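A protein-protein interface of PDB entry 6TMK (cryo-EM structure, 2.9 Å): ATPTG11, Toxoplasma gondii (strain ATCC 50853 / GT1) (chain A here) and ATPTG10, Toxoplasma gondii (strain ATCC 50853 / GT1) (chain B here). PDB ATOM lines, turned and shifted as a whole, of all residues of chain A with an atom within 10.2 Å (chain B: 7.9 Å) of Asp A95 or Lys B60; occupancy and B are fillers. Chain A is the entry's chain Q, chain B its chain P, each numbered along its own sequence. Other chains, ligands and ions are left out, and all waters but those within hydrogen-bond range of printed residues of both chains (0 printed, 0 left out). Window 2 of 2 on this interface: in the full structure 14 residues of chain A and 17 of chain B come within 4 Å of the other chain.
Of the printed residues of chain B, Val A91 touches Ala B56 (3.8 Å) and Leu B59 (3.8 Å). Asp A95 touches one residue of chain B. No residue of chain B comes within 4 Å of Pro A96. Ala A97 touches none of the printed residues of chain B. Printed residues of chain B within 4 Å of Phe A98: Leu B59 (3.2 Å) and Pro B63 (3.9 Å). Ala B56 touches two residues of chain A. Of the printed residues of chain A, Leu B59 touches Val A91 (3.8 Å), Leu A92 (3.9 Å) and Phe A98 (3.2 Å). No residue of chain A comes within 4 Å of Ala B61. Pro B63 touches just one residue of chain A: Phe A98 (3.9 Å). The nearest residue of chain B that does not touch Asp A95 is Leu B59 (6.1 Å). The nearest residue of chain A that does not touch Lys B60 is Val A91 (4.7 Å). The nearest printed residue of chain A that does not touch Leu B59 is Val A88 (4.01 Å).
Printed residues of chain A that touch a printed residue of chain B: Ser A87, Val A91, Leu A92, Asp A95 and Phe A98. Among the printed residues, 7 pairs touch across the chains. Among the printed residues, no Asp or Glu carboxylate lies within 4 Å of a Lys or Arg side-chain nitrogen of the other chain.
Ala B56 touches Ser A87 (CB to OG, 3.9 Å). Val A91 touches Ala B56 (CG2 to CB, 3.8 Å). Leu B59 touches Val A91. Leu A92 touches Leu B59. CG of Lys B60 touches OD1 of Asp A95, at 3.8 Å. Phe A98 touches Leu B59 (CZ to O, 3.2 Å). Pro B63 touches Phe A98 (CD to CZ, 3.9 Å).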
ATOM      1  N   SER A  87     -12.799 -20.358 -22.279  1.00  0.00           N
ATOM      2  CA  SER A  87     -13.008 -21.754 -22.659  1.00  0.00           C
ATOM      3  C   SER A  87     -14.497 -22.061 -22.791  1.00  0.00           C
ATOM      4  O   SER A  87     -14.925 -22.725 -23.746  1.00  0.00           O
ATOM      5  CB  SER A  87     -12.359 -22.680 -21.637  1.00  0.00           C
ATOM      6  OG  SER A  87     -13.033 -22.606 -20.398  1.00  0.00           O
ATOM      7  N   VAL A  88     -15.305 -21.562 -21.856  1.00  0.00           N
ATOM      8  CA  VAL A  88     -16.742 -21.793 -21.909  1.00  0.00           C
ATOM      9  C   VAL A  88     -17.351 -21.078 -23.104  1.00  0.00           C
ATOM     10  O   VAL A  88     -18.269 -21.595 -23.750  1.00  0.00           O
ATOM     11  CB  VAL A  88     -17.398 -21.344 -20.594  1.00  0.00           C
ATOM     12  CG1 VAL A  88     -18.895 -21.322 -20.739  1.00  0.00           C
ATOM     13  CG2 VAL A  88     -16.992 -22.262 -19.472  1.00  0.00           C
ATOM     14  N   ALA A  89     -16.872 -19.869 -23.406  1.00  0.00           N
ATOM     15  CA  ALA A  89     -17.382 -19.160 -24.574  1.00  0.00           C
ATOM     16  C   ALA A  89     -17.117 -19.954 -25.844  1.00  0.00           C
ATOM     17  O   ALA A  89     -17.999 -20.084 -26.704  1.00  0.00           O
ATOM     18  CB  ALA A  89     -16.747 -17.775 -24.662  1.00  0.00           C
ATOM     19  N   GLU A  90     -15.908 -20.506 -25.973  1.00  0.00           N
ATOM     20  CA  GLU A  90     -15.590 -21.316 -27.141  1.00  0.00           C
ATOM     21  C   GLU A  90     -16.489 -22.541 -27.218  1.00  0.00           C
ATOM     22  O   GLU A  90     -17.015 -22.871 -28.288  1.00  0.00           O
ATOM     23  CB  GLU A  90     -14.122 -21.736 -27.098  1.00  0.00           C
ATOM     24  CG  GLU A  90     -13.643 -22.443 -28.355  1.00  0.00           C
ATOM     25  CD  GLU A  90     -13.526 -23.946 -28.178  1.00  0.00           C
ATOM     26  OE1 GLU A  90     -13.106 -24.389 -27.088  1.00  0.00           O
ATOM     27  OE2 GLU A  90     -13.856 -24.684 -29.129  1.00  0.00           O
ATOM     28  N   VAL A  91     -16.691 -23.219 -26.089  1.00  0.00           N
ATOM     29  CA  VAL A  91     -17.535 -24.411 -26.087  1.00  0.00           C
ATOM     30  C   VAL A  91     -18.949 -24.060 -26.530  1.00  0.00           C
ATOM     31  O   VAL A  91     -19.533 -24.723 -27.399  1.00  0.00           O
ATOM     32  CB  VAL A  91     -17.533 -25.062 -24.693  1.00  0.00           C
ATOM     33  CG1 VAL A  91     -18.701 -26.009 -24.553  1.00  0.00           C
ATOM     34  CG2 VAL A  91     -16.232 -25.792 -24.455  1.00  0.00           C
ATOM     35  N   LEU A  92     -19.512 -23.001 -25.950  1.00  0.00           N
ATOM     36  CA  LEU A  92     -20.884 -22.618 -26.264  1.00  0.00           C
ATOM     37  C   LEU A  92     -21.028 -22.237 -27.730  1.00  0.00           C
ATOM     38  O   LEU A  92     -21.978 -22.656 -28.400  1.00  0.00           O
ATOM     39  CB  LEU A  92     -21.322 -21.457 -25.371  1.00  0.00           C
ATOM     40  CG  LEU A  92     -21.500 -21.754 -23.884  1.00  0.00           C
ATOM     41  CD1 LEU A  92     -21.842 -20.484 -23.137  1.00  0.00           C
ATOM     42  CD2 LEU A  92     -22.568 -22.798 -23.666  1.00  0.00           C
ATOM     43  N   GLU A  93     -20.093 -21.440 -28.251  1.00  0.00           N
ATOM     44  CA  GLU A  93     -20.239 -20.972 -29.623  1.00  0.00           C
ATOM     45  C   GLU A  93     -20.001 -22.092 -30.624  1.00  0.00           C
ATOM     46  O   GLU A  93     -20.591 -22.078 -31.710  1.00  0.00           O
ATOM     47  CB  GLU A  93     -19.291 -19.802 -29.893  1.00  0.00           C
ATOM     48  CG  GLU A  93     -17.815 -20.150 -29.833  1.00  0.00           C
ATOM     49  CD  GLU A  93     -17.266 -20.647 -31.159  1.00  0.00           C
ATOM     50  OE1 GLU A  93     -18.014 -20.645 -32.158  1.00  0.00           O
ATOM     51  OE2 GLU A  93     -16.081 -21.042 -31.200  1.00  0.00           O
ATOM     52  N   SER A  94     -19.158 -23.071 -30.290  1.00  0.00           N
ATOM     53  CA  SER A  94     -18.800 -24.098 -31.261  1.00  0.00           C
ATOM     54  C   SER A  94     -19.760 -25.284 -31.219  1.00  0.00           C
ATOM     55  O   SER A  94     -20.371 -25.629 -32.235  1.00  0.00           O
ATOM     56  CB  SER A  94     -17.363 -24.570 -31.015  1.00  0.00           C
ATOM     57  OG  SER A  94     -17.135 -25.835 -31.613  1.00  0.00           O
ATOM     58  N   ASP A  95     -19.905 -25.916 -30.061  1.00  0.00           N
ATOM     59  CA  ASP A  95     -20.631 -27.179 -30.004  1.00  0.00           C
ATOM     60  C   ASP A  95     -22.108 -26.970 -30.329  1.00  0.00           C
ATOM     61  O   ASP A  95     -22.764 -26.133 -29.699  1.00  0.00           O
ATOM     62  CB  ASP A  95     -20.481 -27.811 -28.625  1.00  0.00           C
ATOM     63  CG  ASP A  95     -19.041 -28.144 -28.293  1.00  0.00           C
ATOM     64  OD1 ASP A  95     -18.694 -28.153 -27.095  1.00  0.00           O
ATOM     65  OD2 ASP A  95     -18.257 -28.397 -29.231  1.00  0.00           O
ATOM     66  N   PRO A  96     -22.666 -27.706 -31.297  1.00  0.00           N
ATOM     67  CA  PRO A  96     -23.978 -27.325 -31.844  1.00  0.00           C
ATOM     68  C   PRO A  96     -25.131 -27.576 -30.889  1.00  0.00           C
ATOM     69  O   PRO A  96     -26.184 -26.943 -31.034  1.00  0.00           O
ATOM     70  CB  PRO A  96     -24.095 -28.200 -33.096  1.00  0.00           C
ATOM     71  CG  PRO A  96     -23.328 -29.426 -32.739  1.00  0.00           C
ATOM     72  CD  PRO A  96     -22.161 -28.944 -31.914  1.00  0.00           C
ATOM     73  N   ALA A  97     -24.966 -28.480 -29.923  1.00  0.00           N
ATOM     74  CA  ALA A  97     -26.051 -28.834 -29.016  1.00  0.00           C
ATOM     75  C   ALA A  97     -26.499 -27.661 -28.156  1.00  0.00           C
ATOM     76  O   ALA A  97     -27.635 -27.661 -27.670  1.00  0.00           O
ATOM     77  CB  ALA A  97     -25.624 -29.995 -28.122  1.00  0.00           C
ATOM     78  N   PHE A  98     -25.637 -26.672 -27.956  1.00  0.00           N
ATOM     79  CA  PHE A  98     -25.959 -25.490 -27.173  1.00  0.00           C
ATOM     80  C   PHE A  98     -26.487 -24.335 -28.011  1.00  0.00           C
ATOM     81  O   PHE A  98     -26.842 -23.297 -27.448  1.00  0.00           O
ATOM     82  CB  PHE A  98     -24.723 -25.030 -26.402  1.00  0.00           C
ATOM     83  CG  PHE A  98     -24.274 -25.998 -25.353  1.00  0.00           C
ATOM     84  CD1 PHE A  98     -24.920 -26.066 -24.134  1.00  0.00           C
ATOM     85  CD2 PHE A  98     -23.210 -26.843 -25.587  1.00  0.00           C
ATOM     86  CE1 PHE A  98     -24.511 -26.957 -23.171  1.00  0.00           C
ATOM     87  CE2 PHE A  98     -22.796 -27.734 -24.627  1.00  0.00           C
ATOM     88  CZ  PHE A  98     -23.448 -27.792 -23.417  1.00  0.00           C
ATOM     89  N   ARG A  99     -26.535 -24.474 -29.335  1.00  0.00           N
ATOM     90  CA  ARG A  99     -27.079 -23.406 -30.167  1.00  0.00           C
ATOM     91  C   ARG A  99     -28.570 -23.203 -29.910  1.00  0.00           C
ATOM     92  O   ARG A  99     -29.033 -22.058 -29.772  1.00  0.00           O
ATOM     93  CB  ARG A  99     -26.815 -23.729 -31.637  1.00  0.00           C
ATOM     94  CG  ARG A  99     -25.375 -23.474 -32.062  1.00  0.00           C
ATOM     95  CD  ARG A  99     -25.206 -23.491 -33.572  1.00  0.00           C
ATOM     96  NE  ARG A  99     -25.255 -24.850 -34.112  1.00  0.00           N
ATOM     97  CZ  ARG A  99     -26.366 -25.484 -34.479  1.00  0.00           C
ATOM     98  NH1 ARG A  99     -27.551 -24.897 -34.369  1.00  0.00           N
ATOM     99  NH2 ARG A  99     -26.291 -26.718 -34.955  1.00  0.00           N
ATOM    100  N   GLN A 100     -29.311 -24.299 -29.714  1.00  0.00           N
ATOM    101  CA  GLN A 100     -30.717 -24.169 -29.353  1.00  0.00           C
ATOM    102  C   GLN A 100     -30.857 -23.559 -27.970  1.00  0.00           C
ATOM    103  O   GLN A 100     -31.760 -22.738 -27.731  1.00  0.00           O
ATOM    104  CB  GLN A 100     -31.399 -25.534 -29.397  1.00  0.00           C
ATOM    105  CG  GLN A 100     -31.229 -26.267 -30.713  1.00  0.00           C
ATOM    106  CD  GLN A 100     -32.409 -27.158 -31.042  1.00  0.00           C
ATOM    107  OE1 GLN A 100     -32.431 -28.337 -30.689  1.00  0.00           O
ATOM    108  NE2 GLN A 100     -33.403 -26.597 -31.723  1.00  0.00           N
ATOM    109  N   ALA A 101     -29.930 -23.875 -27.071  1.00  0.00           N
ATOM    110  CA  ALA A 101     -30.105 -23.406 -25.713  1.00  0.00           C
ATOM    111  C   ALA A 101     -29.794 -21.926 -25.669  1.00  0.00           C
ATOM    112  O   ALA A 101     -30.421 -21.179 -24.911  1.00  0.00           O
ATOM    113  CB  ALA A 101     -29.205 -24.185 -24.761  1.00  0.00           C
ATOM    114  N   ARG A 102     -28.826 -21.485 -26.476  1.00  0.00           N
ATOM    115  CA  ARG A 102     -28.530 -20.066 -26.518  1.00  0.00           C
ATOM    116  C   ARG A 102     -29.743 -19.324 -27.053  1.00  0.00           C
ATOM    117  O   ARG A 102     -30.183 -18.328 -26.467  1.00  0.00           O
ATOM    118  CB  ARG A 102     -27.297 -19.794 -27.381  1.00  0.00           C
ATOM    119  CG  ARG A 102     -25.983 -19.883 -26.622  1.00  0.00           C
ATOM    120  CD  ARG A 102     -24.828 -19.317 -27.433  1.00  0.00           C
ATOM    121  NE  ARG A 102     -24.702 -19.942 -28.747  1.00  0.00           N
ATOM    122  CZ  ARG A 102     -23.795 -19.592 -29.654  1.00  0.00           C
ATOM    123  NH1 ARG A 102     -22.924 -18.628 -29.391  1.00  0.00           N
ATOM    124  NH2 ARG A 102     -23.755 -20.211 -30.825  1.00  0.00           N
ATOM    125  N   ASN A 103     -30.307 -19.799 -28.169  1.00  0.00           N
ATOM    126  CA  ASN A 103     -31.503 -19.129 -28.685  1.00  0.00           C
ATOM    127  C   ASN A 103     -32.763 -19.804 -28.146  1.00  0.00           C
ATOM    128  O   ASN A 103     -33.696 -20.113 -28.886  1.00  0.00           O
ATOM    129  CB  ASN A 103     -31.504 -19.100 -30.210  1.00  0.00           C
ATOM    130  CG  ASN A 103     -31.675 -20.467 -30.819  1.00  0.00           C
ATOM    131  OD1 ASN A 103     -31.269 -21.461 -30.241  1.00  0.00           O
ATOM    132  ND2 ASN A 103     -32.289 -20.521 -31.995  1.00  0.00           N
ATOM    133  N   ASP B  55     -16.790 -25.207 -15.957  1.00  0.00           N
ATOM    134  CA  ASP B  55     -15.896 -26.279 -16.378  1.00  0.00           C
ATOM    135  C   ASP B  55     -16.271 -26.711 -17.793  1.00  0.00           C
ATOM    136  O   ASP B  55     -17.339 -27.294 -18.017  1.00  0.00           O
ATOM    137  CB  ASP B  55     -15.957 -27.450 -15.403  1.00  0.00           C
ATOM    138  CG  ASP B  55     -14.701 -28.294 -15.431  1.00  0.00           C
ATOM    139  OD1 ASP B  55     -14.038 -28.340 -16.487  1.00  0.00           O
ATOM    140  OD2 ASP B  55     -14.372 -28.905 -14.395  1.00  0.00           O
ATOM    141  N   ALA B  56     -15.379 -26.425 -18.743  1.00  0.00           N
ATOM    142  CA  ALA B  56     -15.658 -26.692 -20.149  1.00  0.00           C
ATOM    143  C   ALA B  56     -15.801 -28.183 -20.416  1.00  0.00           C
ATOM    144  O   ALA B  56     -16.633 -28.597 -21.230  1.00  0.00           O
ATOM    145  CB  ALA B  56     -14.551 -26.106 -21.017  1.00  0.00           C
ATOM    146  N   ASP B  57     -15.001 -29.007 -19.740  1.00  0.00           N
ATOM    147  CA  ASP B  57     -15.068 -30.447 -19.955  1.00  0.00           C
ATOM    148  C   ASP B  57     -16.432 -30.992 -19.550  1.00  0.00           C
ATOM    149  O   ASP B  57     -17.066 -31.745 -20.300  1.00  0.00           O
ATOM    150  CB  ASP B  57     -13.955 -31.133 -19.169  1.00  0.00           C
ATOM    151  CG  ASP B  57     -12.577 -30.643 -19.564  1.00  0.00           C
ATOM    152  OD1 ASP B  57     -12.228 -30.738 -20.760  1.00  0.00           O
ATOM    153  OD2 ASP B  57     -11.841 -30.162 -18.677  1.00  0.00           O
ATOM    154  N   VAL B  58     -16.903 -30.611 -18.365  1.00  0.00           N
ATOM    155  CA  VAL B  58     -18.191 -31.094 -17.887  1.00  0.00           C
ATOM    156  C   VAL B  58     -19.315 -30.532 -18.742  1.00  0.00           C
ATOM    157  O   VAL B  58     -20.305 -31.219 -19.027  1.00  0.00           O
ATOM    158  CB  VAL B  58     -18.374 -30.724 -16.406  1.00  0.00           C
ATOM    159  CG1 VAL B  58     -19.610 -31.383 -15.847  1.00  0.00           C
ATOM    160  CG2 VAL B  58     -17.151 -31.108 -15.611  1.00  0.00           C
ATOM    161  N   LEU B  59     -19.180 -29.279 -19.172  1.00  0.00           N
ATOM    162  CA  LEU B  59     -20.186 -28.688 -20.042  1.00  0.00           C
ATOM    163  C   LEU B  59     -20.280 -29.442 -21.361  1.00  0.00           C
ATOM    164  O   LEU B  59     -21.379 -29.685 -21.872  1.00  0.00           O
ATOM    165  CB  LEU B  59     -19.849 -27.220 -20.280  1.00  0.00           C
ATOM    166  CG  LEU B  59     -20.913 -26.365 -20.948  1.00  0.00           C
ATOM    167  CD1 LEU B  59     -22.090 -26.195 -20.032  1.00  0.00           C
ATOM    168  CD2 LEU B  59     -20.326 -25.024 -21.298  1.00  0.00           C
ATOM    169  N   LYS B  60     -19.135 -29.823 -21.923  1.00  0.00           N
ATOM    170  CA  LYS B  60     -19.125 -30.585 -23.165  1.00  0.00           C
ATOM    171  C   LYS B  60     -19.688 -31.986 -22.965  1.00  0.00           C
ATOM    172  O   LYS B  60     -20.347 -32.528 -23.859  1.00  0.00           O
ATOM    173  CB  LYS B  60     -17.700 -30.658 -23.704  1.00  0.00           C
ATOM    174  CG  LYS B  60     -17.588 -31.168 -25.119  1.00  0.00           C
ATOM    175  CD  LYS B  60     -16.160 -31.061 -25.617  1.00  0.00           C
ATOM    176  CE  LYS B  60     -15.838 -32.164 -26.611  1.00  0.00           C
ATOM    177  NZ  LYS B  60     -15.345 -33.396 -25.941  1.00  0.00           N
ATOM    178  N   ALA B  61     -19.442 -32.587 -21.801  1.00  0.00           N
ATOM    179  CA  ALA B  61     -19.910 -33.943 -21.547  1.00  0.00           C
ATOM    180  C   ALA B  61     -21.375 -34.008 -21.146  1.00  0.00           C
ATOM    181  O   ALA B  61     -21.963 -35.094 -21.181  1.00  0.00           O
ATOM    182  CB  ALA B  61     -19.068 -34.588 -20.452  1.00  0.00           C
ATOM    183  N   LEU B  62     -21.975 -32.885 -20.762  1.00  0.00           N
ATOM    184  CA  LEU B  62     -23.385 -32.897 -20.372  1.00  0.00           C
ATOM    185  C   LEU B  62     -24.290 -33.427 -21.475  1.00  0.00           C
ATOM    186  O   LEU B  62     -25.032 -34.398 -21.234  1.00  0.00           O
ATOM    187  CB  LEU B  62     -23.784 -31.489 -19.933  1.00  0.00           C
ATOM    188  CG  LEU B  62     -25.246 -31.255 -19.588  1.00  0.00           C
ATOM    189  CD1 LEU B  62     -25.592 -31.937 -18.294  1.00  0.00           C
ATOM    190  CD2 LEU B  62     -25.505 -29.780 -19.481  1.00  0.00           C
ATOM    191  N   PRO B  63     -24.299 -32.856 -22.683  1.00  0.00           N
ATOM    192  CA  PRO B  63     -25.175 -33.396 -23.730  1.00  0.00           C
ATOM    193  C   PRO B  63     -24.801 -34.800 -24.159  1.00  0.00           C
ATOM    194  O   PRO B  63     -25.657 -35.513 -24.695  1.00  0.00           O
ATOM    195  CB  PRO B  63     -25.003 -32.392 -24.876  1.00  0.00           C
ATOM    196  CG  PRO B  63     -23.677 -31.792 -24.647  1.00  0.00           C
ATOM    197  CD  PRO B  63     -23.538 -31.695 -23.166  1.00  0.00           C
ATOM    198  N   GLN B  64     -23.554 -35.219 -23.945  1.00  0.00           N
ATOM    199  CA  GLN B  64     -23.186 -36.602 -24.212  1.00  0.00           C
ATOM    200  C   GLN B  64     -23.824 -37.535 -23.195  1.00  0.00           C
ATOM    201  O   GLN B  64     -24.324 -38.607 -23.552  1.00  0.00           O
ATOM    202  CB  GLN B  64     -21.669 -36.754 -24.202  1.00  0.00           C
ATOM    203  CG  GLN B  64     -20.941 -35.791 -25.110  1.00  0.00           C
ATOM    204  CD  GLN B  64     -19.514 -36.209 -25.369  1.00  0.00           C
ATOM    205  OE1 GLN B  64     -19.259 -37.208 -26.039  1.00  0.00           O
ATOM    206  NE2 GLN B  64     -18.572 -35.446 -24.834  1.00  0.00           N
ATOM    207  N   TYR B  65     -23.812 -37.145 -21.919  1.00  0.00           N
ATOM    208  CA  TYR B  65     -24.472 -37.949 -20.899  1.00  0.00           C
ATOM    209  C   TYR B  65     -25.969 -38.015 -21.146  1.00  0.00           C
ATOM    210  O   TYR B  65     -26.595 -39.060 -20.942  1.00  0.00           O
ATOM    211  CB  TYR B  65     -24.201 -37.383 -19.508  1.00  0.00           C
ATOM    212  CG  TYR B  65     -25.095 -37.999 -18.464  1.00  0.00           C
ATOM    213  CD1 TYR B  65     -24.906 -39.306 -18.049  1.00  0.00           C
ATOM    214  CD2 TYR B  65     -26.148 -37.287 -17.919  1.00  0.00           C
ATOM    215  CE1 TYR B  65     -25.728 -39.879 -17.112  1.00  0.00           C
ATOM    216  CE2 TYR B  65     -26.974 -37.852 -16.982  1.00  0.00           C
ATOM    217  CZ  TYR B  65     -26.759 -39.149 -16.580  1.00  0.00           C
ATOM    218  OH  TYR B  65     -27.580 -39.728 -15.646  1.00  0.00           O
ATOM    219  N   TRP B 101     -25.141 -31.941 -13.111  1.00  0.00           N
ATOM    220  CA  TRP B 101     -23.753 -31.507 -13.173  1.00  0.00           C
ATOM    221  C   TRP B 101     -22.824 -32.585 -12.634  1.00  0.00           C
ATOM    222  O   TRP B 101     -21.790 -32.896 -13.241  1.00  0.00           O
ATOM    223  CB  TRP B 101     -23.591 -30.213 -12.383  1.00  0.00           C
ATOM    224  CG  TRP B 101     -22.357 -29.460 -12.712  1.00  0.00           C
ATOM    225  CD1 TRP B 101     -21.332 -29.168 -11.873  1.00  0.00           C
ATOM    226  CD2 TRP B 101     -22.020 -28.887 -13.975  1.00  0.00           C
ATOM    227  NE1 TRP B 101     -20.371 -28.454 -12.534  1.00  0.00           N
ATOM    228  CE2 TRP B 101     -20.770 -28.269 -13.829  1.00  0.00           C
ATOM    229  CE3 TRP B 101     -22.653 -28.842 -15.217  1.00  0.00           C
ATOM    230  CZ2 TRP B 101     -20.141 -27.613 -14.873  1.00  0.00           C
ATOM    231  CZ3 TRP B 101     -22.026 -28.192 -16.250  1.00  0.00           C
ATOM    232  CH2 TRP B 101     -20.785 -27.585 -16.075  1.00  0.00           C
ATOM    233  N   ALA B 104     -22.630 -35.403 -15.113  1.00  0.00           N
ATOM    234  CA  ALA B 104     -21.806 -35.056 -16.264  1.00  0.00           C
ATOM    235  C   ALA B 104     -20.327 -35.125 -15.921  1.00  0.00           C
ATOM    236  O   ALA B 104     -19.510 -35.568 -16.736  1.00  0.00           O
ATOM    237  CB  ALA B 104     -22.177 -33.665 -16.755  1.00  0.00           C
ATOM    238  N   PHE B 107     -19.428 -38.691 -15.885  1.00  0.00           N
ATOM    239  CA  PHE B 107     -19.402 -39.189 -17.254  1.00  0.00           C
ATOM    240  C   PHE B 107     -18.104 -38.810 -17.948  1.00  0.00           C
ATOM    241  O   PHE B 107     -17.523 -39.615 -18.683  1.00  0.00           O
ATOM    242  CB  PHE B 107     -20.603 -38.646 -18.022  1.00  0.00           C
ATOM    243  CG  PHE B 107     -20.727 -39.184 -19.413  1.00  0.00           C
ATOM    244  CD1 PHE B 107     -21.402 -40.363 -19.654  1.00  0.00           C
ATOM    245  CD2 PHE B 107     -20.172 -38.509 -20.479  1.00  0.00           C
ATOM    246  CE1 PHE B 107     -21.514 -40.859 -20.930  1.00  0.00           C
ATOM    247  CE2 PHE B 107     -20.281 -39.002 -21.754  1.00  0.00           C
ATOM    248  CZ  PHE B 107     -20.954 -40.179 -21.981  1.00  0.00           C
ATOM    249  N   SER B 108     -17.642 -37.579 -17.739  1.00  0.00           N
ATOM    250  CA  SER B 108     -16.378 -37.157 -18.328  1.00  0.00           C
ATOM    251  C   SER B 108     -15.235 -38.013 -17.804  1.00  0.00           C
ATOM    252  O   SER B 108     -14.410 -38.523 -18.579  1.00  0.00           O
ATOM    253  CB  SER B 108     -16.134 -35.681 -18.026  1.00  0.00           C
ATOM    254  OG  SER B 108     -15.853 -35.481 -16.659  1.00  0.00           O
ATOM    255  N   GLN B 111     -15.492 -41.563 -19.390  1.00  0.00           N
ATOM    256  CA  GLN B 111     -15.129 -41.695 -20.793  1.00  0.00           C
ATOM    257  C   GLN B 111     -13.659 -41.392 -21.032  1.00  0.00           C
ATOM    258  O   GLN B 111     -13.114 -41.815 -22.055  1.00  0.00           O
ATOM    259  CB  GLN B 111     -16.002 -40.795 -21.666  1.00  0.00           C
ATOM    260  CG  GLN B 111     -15.756 -39.320 -21.509  1.00  0.00           C
ATOM    261  CD  GLN B 111     -16.654 -38.497 -22.404  1.00  0.00           C
ATOM    262  OE1 GLN B 111     -17.502 -39.034 -23.115  1.00  0.00           O
ATOM    263  NE2 GLN B 111     -16.468 -37.183 -22.383  1.00  0.00           N
